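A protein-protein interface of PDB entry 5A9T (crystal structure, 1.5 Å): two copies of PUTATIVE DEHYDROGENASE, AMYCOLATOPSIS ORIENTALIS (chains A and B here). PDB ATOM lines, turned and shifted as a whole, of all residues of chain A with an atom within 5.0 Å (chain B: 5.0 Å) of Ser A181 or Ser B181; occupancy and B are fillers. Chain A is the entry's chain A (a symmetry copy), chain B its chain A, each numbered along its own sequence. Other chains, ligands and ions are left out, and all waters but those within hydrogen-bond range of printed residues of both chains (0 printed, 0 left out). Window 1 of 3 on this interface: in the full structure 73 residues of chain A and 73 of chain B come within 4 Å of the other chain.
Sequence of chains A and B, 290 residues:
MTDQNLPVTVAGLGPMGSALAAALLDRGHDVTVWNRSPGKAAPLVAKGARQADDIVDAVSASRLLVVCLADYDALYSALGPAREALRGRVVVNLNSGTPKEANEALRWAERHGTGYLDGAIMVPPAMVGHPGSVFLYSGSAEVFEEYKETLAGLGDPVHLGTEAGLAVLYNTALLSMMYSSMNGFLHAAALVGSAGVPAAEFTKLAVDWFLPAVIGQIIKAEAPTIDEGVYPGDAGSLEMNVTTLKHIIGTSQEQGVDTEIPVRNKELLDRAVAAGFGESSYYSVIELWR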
ATOM      1  N   MET A 177     -28.861   7.551  -6.267  1.00  0.00           N
ATOM      2  CA  MET A 177     -27.596   6.841  -6.184  1.00  0.00           C
ATOM      3  C   MET A 177     -26.495   7.659  -6.872  1.00  0.00           C
ATOM      4  O   MET A 177     -25.335   7.717  -6.334  1.00  0.00           O
ATOM      5  CB  MET A 177     -27.723   5.479  -6.815  1.00  0.00           C
ATOM      6  CG  MET A 177     -26.393   4.738  -6.880  1.00  0.00           C
ATOM      7  SD  MET A 177     -26.746   3.070  -7.605  1.00  0.00           S
ATOM      8  CE  MET A 177     -25.184   2.435  -8.233  1.00  0.00           C
ATOM      9  N   MET A 178     -26.765   8.254  -8.021  1.00  0.00           N
ATOM     10  CA  MET A 178     -25.773   9.046  -8.759  1.00  0.00           C
ATOM     11  C   MET A 178     -25.294  10.228  -7.936  1.00  0.00           C
ATOM     12  O   MET A 178     -24.093  10.546  -7.852  1.00  0.00           O
ATOM     13  CB  MET A 178     -26.333   9.480 -10.074  1.00  0.00           C
ATOM     14  CG  MET A 178     -25.286  10.238 -10.831  1.00  0.00           C
ATOM     15  SD  MET A 178     -25.815  10.402 -12.549  1.00  0.00           S
ATOM     16  CE  MET A 178     -24.479  11.471 -13.178  1.00  0.00           C
ATOM     17  N   TYR A 179     -26.206  10.964  -7.288  1.00  0.00           N
ATOM     18  CA  TYR A 179     -25.765  12.170  -6.540  1.00  0.00           C
ATOM     19  C   TYR A 179     -24.810  11.772  -5.425  1.00  0.00           C
ATOM     20  O   TYR A 179     -23.722  12.349  -5.225  1.00  0.00           O
ATOM     21  CB  TYR A 179     -26.923  12.993  -5.966  1.00  0.00           C
ATOM     22  CG  TYR A 179     -27.638  13.835  -6.978  1.00  0.00           C
ATOM     23  CD1 TYR A 179     -26.969  14.944  -7.516  1.00  0.00           C
ATOM     24  CD2 TYR A 179     -28.904  13.505  -7.461  1.00  0.00           C
ATOM     25  CE1 TYR A 179     -27.572  15.712  -8.488  1.00  0.00           C
ATOM     26  CE2 TYR A 179     -29.496  14.223  -8.440  1.00  0.00           C
ATOM     27  CZ  TYR A 179     -28.808  15.320  -8.965  1.00  0.00           C
ATOM     28  OH  TYR A 179     -29.456  16.036  -9.987  1.00  0.00           O
ATOM     29  N   SER A 180     -25.165  10.704  -4.690  1.00  0.00           N
ATOM     30  CA  SER A 180     -24.282  10.278  -3.562  1.00  0.00           C
ATOM     31  C   SER A 180     -22.933   9.761  -4.093  1.00  0.00           C
ATOM     32  O   SER A 180     -21.859  10.039  -3.535  1.00  0.00           O
ATOM     33  CB  SER A 180     -24.982   9.187  -2.791  1.00  0.00           C
ATOM     34  OG  SER A 180     -25.972   9.720  -1.964  1.00  0.00           O
ATOM     35  N   SER A 181     -22.989   8.932  -5.130  1.00  0.00           N
ATOM     36  CA  SER A 181     -21.745   8.405  -5.735  1.00  0.00           C
ATOM     37  C   SER A 181     -20.847   9.475  -6.277  1.00  0.00           C
ATOM     38  O   SER A 181     -19.595   9.474  -6.067  1.00  0.00           O
ATOM     39  CB  SER A 181     -22.134   7.445  -6.876  1.00  0.00           C
ATOM     40  OG  SER A 181     -22.849   6.368  -6.327  1.00  0.00           O
ATOM     41  N   MET A 182     -21.380  10.486  -6.945  1.00  0.00           N
ATOM     42  CA  MET A 182     -20.620  11.551  -7.485  1.00  0.00           C
ATOM     43  C   MET A 182     -20.004  12.372  -6.357  1.00  0.00           C
ATOM     44  O   MET A 182     -18.862  12.734  -6.459  1.00  0.00           O
ATOM     45  CB  MET A 182     -21.458  12.505  -8.357  1.00  0.00           C
ATOM     46  CG  MET A 182     -20.712  13.570  -9.044  1.00  0.00           C
ATOM     47  SD  MET A 182     -19.539  12.821 -10.237  1.00  0.00           S
ATOM     48  CE  MET A 182     -20.554  11.846 -10.945  1.00  0.00           C
ATOM     49  N   ASN A 183     -20.768  12.620  -5.300  1.00  0.00           N
ATOM     50  CA  ASN A 183     -20.212  13.354  -4.159  1.00  0.00           C
ATOM     51  C   ASN A 183     -19.027  12.581  -3.564  1.00  0.00           C
ATOM     52  O   ASN A 183     -18.058  13.183  -3.111  1.00  0.00           O
ATOM     53  CB  ASN A 183     -21.315  13.681  -3.148  1.00  0.00           C
ATOM     54  CG  ASN A 183     -22.310  14.694  -3.658  1.00  0.00           C
ATOM     55  OD1 ASN A 183     -23.443  14.717  -3.077  1.00  0.00           O
ATOM     56  ND2 ASN A 183     -22.027  15.347  -4.657  1.00  0.00           N
ATOM     57  N   GLY A 184     -19.208  11.260  -3.399  1.00  0.00           N
ATOM     58  CA  GLY A 184     -18.125  10.436  -2.921  1.00  0.00           C
ATOM     59  C   GLY A 184     -16.911  10.517  -3.787  1.00  0.00           C
ATOM     60  O   GLY A 184     -15.784  10.688  -3.277  1.00  0.00           O
ATOM     61  N   PHE A 185     -17.080  10.449  -5.110  1.00  0.00           N
ATOM     62  CA  PHE A 185     -15.936  10.630  -5.975  1.00  0.00           C
ATOM     63  C   PHE A 185     -15.267  11.986  -5.786  1.00  0.00           C
ATOM     64  O   PHE A 185     -14.041  12.072  -5.778  1.00  0.00           O
ATOM     65  CB  PHE A 185     -16.294  10.391  -7.451  1.00  0.00           C
ATOM     66  CG  PHE A 185     -15.208  10.805  -8.357  1.00  0.00           C
ATOM     67  CD1 PHE A 185     -14.123   9.924  -8.598  1.00  0.00           C
ATOM     68  CD2 PHE A 185     -15.159  12.050  -8.935  1.00  0.00           C
ATOM     69  CE1 PHE A 185     -13.042  10.350  -9.351  1.00  0.00           C
ATOM     70  CE2 PHE A 185     -14.088  12.438  -9.715  1.00  0.00           C
ATOM     71  CZ  PHE A 185     -13.010  11.640  -9.877  1.00  0.00           C
ATOM     72  N   LEU A 211     -14.451   1.436  -8.769  1.00  0.00           N
ATOM     73  CA  LEU A 211     -15.889   1.493  -8.915  1.00  0.00           C
ATOM     74  C   LEU A 211     -16.551   0.157  -9.282  1.00  0.00           C
ATOM     75  O   LEU A 211     -17.398  -0.321  -8.537  1.00  0.00           O
ATOM     76  CB  LEU A 211     -16.248   2.677  -9.807  1.00  0.00           C
ATOM     77  CG  LEU A 211     -17.727   3.020  -9.926  1.00  0.00           C
ATOM     78  CD1 LEU A 211     -18.320   3.568  -8.646  1.00  0.00           C
ATOM     79  CD2 LEU A 211     -17.886   3.979 -11.053  1.00  0.00           C
ATOM     80  N   ILE A 215     -16.588  -1.599  -5.432  1.00  0.00           N
ATOM     81  CA  ILE A 215     -17.925  -1.156  -4.990  1.00  0.00           C
ATOM     82  C   ILE A 215     -18.986  -2.063  -5.614  1.00  0.00           C
ATOM     83  O   ILE A 215     -19.869  -2.595  -4.924  1.00  0.00           O
ATOM     84  CB  ILE A 215     -18.086   0.344  -5.338  1.00  0.00           C
ATOM     85  CG1 ILE A 215     -17.082   1.211  -4.519  1.00  0.00           C
ATOM     86  CG2 ILE A 215     -19.529   0.744  -4.957  1.00  0.00           C
ATOM     87  CD1 ILE A 215     -17.058   2.660  -4.902  1.00  0.00           C
ATOM     88  N   MET B 177     -15.130   7.486  -0.910  1.00  0.00           N
ATOM     89  CA  MET B 177     -15.975   7.313  -2.079  1.00  0.00           C
ATOM     90  C   MET B 177     -16.885   6.093  -1.886  1.00  0.00           C
ATOM     91  O   MET B 177     -18.104   6.158  -2.273  1.00  0.00           O
ATOM     92  CB  MET B 177     -15.127   7.157  -3.314  1.00  0.00           C
ATOM     93  CG  MET B 177     -15.953   6.837  -4.555  1.00  0.00           C
ATOM     94  SD  MET B 177     -14.770   6.758  -5.977  1.00  0.00           S
ATOM     95  CE  MET B 177     -15.586   5.824  -7.280  1.00  0.00           C
ATOM     96  N   MET B 178     -16.376   4.994  -1.357  1.00  0.00           N
ATOM     97  CA  MET B 178     -17.164   3.773  -1.146  1.00  0.00           C
ATOM     98  C   MET B 178     -18.326   4.028  -0.202  1.00  0.00           C
ATOM     99  O   MET B 178     -19.474   3.600  -0.421  1.00  0.00           O
ATOM    100  CB  MET B 178     -16.286   2.669  -0.654  1.00  0.00           C
ATOM    101  CG  MET B 178     -17.100   1.422  -0.500  1.00  0.00           C
ATOM    102  SD  MET B 178     -15.982   0.018  -0.307  1.00  0.00           S
ATOM    103  CE  MET B 178     -17.200  -1.299   0.017  1.00  0.00           C
ATOM    104  N   TYR B 179     -18.095   4.728   0.916  1.00  0.00           N
ATOM    105  CA  TYR B 179     -19.202   4.922   1.889  1.00  0.00           C
ATOM    106  C   TYR B 179     -20.337   5.699   1.241  1.00  0.00           C
ATOM    107  O   TYR B 179     -21.531   5.345   1.316  1.00  0.00           O
ATOM    108  CB  TYR B 179     -18.765   5.617   3.183  1.00  0.00           C
ATOM    109  CG  TYR B 179     -18.028   4.729   4.138  1.00  0.00           C
ATOM    110  CD1 TYR B 179     -18.743   3.715   4.793  1.00  0.00           C
ATOM    111  CD2 TYR B 179     -16.651   4.824   4.332  1.00  0.00           C
ATOM    112  CE1 TYR B 179     -18.090   2.844   5.638  1.00  0.00           C
ATOM    113  CE2 TYR B 179     -15.987   3.956   5.127  1.00  0.00           C
ATOM    114  CZ  TYR B 179     -16.718   2.950   5.764  1.00  0.00           C
ATOM    115  OH  TYR B 179     -15.989   2.064   6.576  1.00  0.00           O
ATOM    116  N   SER B 180     -19.983   6.771   0.510  1.00  0.00           N
ATOM    117  CA  SER B 180     -21.054   7.592  -0.131  1.00  0.00           C
ATOM    118  C   SER B 180     -21.775   6.787  -1.227  1.00  0.00           C
ATOM    119  O   SER B 180     -23.006   6.840  -1.377  1.00  0.00           O
ATOM    120  CB  SER B 180     -20.421   8.822  -0.732  1.00  0.00           C
ATOM    121  OG  SER B 180     -20.132   9.764   0.256  1.00  0.00           O
ATOM    122  N   SER B 181     -20.998   6.098  -2.056  1.00  0.00           N
ATOM    123  CA  SER B 181     -21.596   5.265  -3.124  1.00  0.00           C
ATOM    124  C   SER B 181     -22.486   4.178  -2.603  1.00  0.00           C
ATOM    125  O   SER B 181     -23.620   3.932  -3.116  1.00  0.00           O
ATOM    126  CB  SER B 181     -20.451   4.633  -3.940  1.00  0.00           C
ATOM    127  OG  SER B 181     -19.715   5.665  -4.545  1.00  0.00           O
ATOM    128  N   MET B 182     -22.107   3.490  -1.537  1.00  0.00           N
ATOM    129  CA  MET B 182     -22.881   2.454  -0.961  1.00  0.00           C
ATOM    130  C   MET B 182     -24.161   3.032  -0.369  1.00  0.00           C
ATOM    131  O   MET B 182     -25.197   2.447  -0.542  1.00  0.00           O
ATOM    132  CB  MET B 182     -22.140   1.705   0.162  1.00  0.00           C
ATOM    133  CG  MET B 182     -22.839   0.541   0.728  1.00  0.00           C
ATOM    134  SD  MET B 182     -23.049  -0.736  -0.570  1.00  0.00           S
ATOM    135  CE  MET B 182     -21.561  -0.757  -1.087  1.00  0.00           C
ATOM    136  N   ASN B 183     -24.061   4.180   0.291  1.00  0.00           N
ATOM    137  CA  ASN B 183     -25.267   4.815   0.832  1.00  0.00           C
ATOM    138  C   ASN B 183     -26.242   5.146  -0.305  1.00  0.00           C
ATOM    139  O   ASN B 183     -27.453   5.054  -0.130  1.00  0.00           O
ATOM    140  CB  ASN B 183     -24.890   6.017   1.703  1.00  0.00           C
ATOM    141  CG  ASN B 183     -24.193   5.631   2.984  1.00  0.00           C
ATOM    142  OD1 ASN B 183     -23.502   6.540   3.549  1.00  0.00           O
ATOM    143  ND2 ASN B 183     -24.229   4.459   3.345  1.00  0.00           N
ATOM    144  N   GLY B 184     -25.703   5.713  -1.398  1.00  0.00           N
ATOM    145  CA  GLY B 184     -26.525   5.989  -2.550  1.00  0.00           C
ATOM    146  C   GLY B 184     -27.197   4.767  -3.085  1.00  0.00           C
ATOM    147  O   GLY B 184     -28.415   4.789  -3.360  1.00  0.00           O
ATOM    148  N   PHE B 185     -26.468   3.656  -3.213  1.00  0.00           N
ATOM    149  CA  PHE B 185     -27.117   2.434  -3.630  1.00  0.00           C
ATOM    150  C   PHE B 185     -28.227   2.005  -2.677  1.00  0.00           C
ATOM    151  O   PHE B 185     -29.283   1.564  -3.122  1.00  0.00           O
ATOM    152  CB  PHE B 185     -26.105   1.297  -3.846  1.00  0.00           C
ATOM    153  CG  PHE B 185     -26.769  -0.006  -4.032  1.00  0.00           C
ATOM    154  CD1 PHE B 185     -27.267  -0.362  -5.311  1.00  0.00           C
ATOM    155  CD2 PHE B 185     -26.995  -0.877  -2.995  1.00  0.00           C
ATOM    156  CE1 PHE B 185     -27.996  -1.528  -5.470  1.00  0.00           C
ATOM    157  CE2 PHE B 185     -27.691  -2.054  -3.186  1.00  0.00           C
ATOM    158  CZ  PHE B 185     -28.246  -2.359  -4.379  1.00  0.00           C
ATOM    159  N   LEU B 211     -23.975   1.887 -12.814  1.00  0.00           N
ATOM    160  CA  LEU B 211     -22.731   2.239 -12.165  1.00  0.00           C
ATOM    161  C   LEU B 211     -21.558   2.499 -13.121  1.00  0.00           C
ATOM    162  O   LEU B 211     -21.003   3.592 -13.111  1.00  0.00           O
ATOM    163  CB  LEU B 211     -22.461   1.244 -11.041  1.00  0.00           C
ATOM    164  CG  LEU B 211     -21.294   1.557 -10.115  1.00  0.00           C
ATOM    165  CD1 LEU B 211     -21.535   2.765  -9.235  1.00  0.00           C
ATOM    166  CD2 LEU B 211     -21.013   0.342  -9.303  1.00  0.00           C
ATOM    167  N   ILE B 215     -22.561   6.444 -14.279  1.00  0.00           N
ATOM    168  CA  ILE B 215     -21.786   7.186 -13.264  1.00  0.00           C
ATOM    169  C   ILE B 215     -20.319   7.238 -13.692  1.00  0.00           C
ATOM    170  O   ILE B 215     -19.691   8.307 -13.721  1.00  0.00           O
ATOM    171  CB  ILE B 215     -22.024   6.525 -11.885  1.00  0.00           C
ATOM    172  CG1 ILE B 215     -23.513   6.678 -11.449  1.00  0.00           C
ATOM    173  CG2 ILE B 215     -21.120   7.260 -10.870  1.00  0.00           C
ATOM    174  CD1 ILE B 215     -23.872   5.935 -10.197  1.00  0.00           C
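Ser A181 touches just one residue of chain B: Ser B181. Of chain A, only Ser A181 (3.6 Å) comes within 4 Å of Ser B181. Of the printed residues of chain A, Phe B185 touches Met A177. Printed residues of chain B within 4 Å of Met A177: Gly B184, Phe B185 and Leu B211. Of the printed residues of chain B, Ile A215 touches Met B178 (3.9 Å). Printed residues of chain B within 4 Å of Leu A211: Met B177 (3.8 Å) and Leu B211 (3.4 Å). Asn A183 touches none of the printed residues of chain B. Tyr A179 touches none of the printed residues of chain B. The nearest residue of chain B that does not touch Ser A181 is Ile B215 (4.03 Å).
The side-chain hydroxyl of Ser B181 is in hydrogen-bond range of the backbone carbonyl oxygen of Met B177. The backbone carbonyl oxygen (O) of Met A177 is in hydrogen-bond range of the side-chain hydroxyl (OG) of Ser A181 (2.8 Å).
Among the printed residues, merely in contact across the chains: Leu A211 with Leu B211, Ser A180 with Ser B180, Ser A180 with Gly B184, Gly A184 with Ser B180, Met A177 with Gly B184, Gly A184 with Met B177, Ser A181 with Ser B181, Met A177 with Leu B211, Leu A211 with Met B177, Met A177 with Phe B185, Phe A185 with Met B177, Ile A215 with Met B178 and Met A178 with Ile B215.
Of the 11 printed residues of chain A, 8 touch a printed residue of chain B. Printed residues of chain A that touch a printed residue of chain B: Met A177, Met A178, Ser A180, Ser A181, Gly A184, Phe A185, Leu A211 and Ile A215. Hydrophobic or aromatic side chains of chain A that line the printed part of chain B: Met A177, Leu A211 and Ile A215. Along chain A the printed residues that touch a printed residue of chain B span positions 177 to 215. Of the 11 printed residues of chain B, 8 touch a printed residue of chain A. Among the printed residues, 13 pairs touch across the chains. Among the printed residues, no Asp or Glu carboxylate lies within 4 Å of a Lys or Arg side-chain nitrogen of the other chain.
Met A177 touches Gly B184, and with the chains exchanged Gly A184 touches Met B177. Met A177 touches Phe B185, and with the chains exchanged Phe A185 touches Met B177. Met A177 touches Leu B211, and with the chains exchanged Leu A211 touches Met B177. Ser A181 touches its own counterpart, Ser B181. Positions printed for both chains: 177, 178, 179, 180, 181, 182, 183, 184, 185, 211 and 215.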
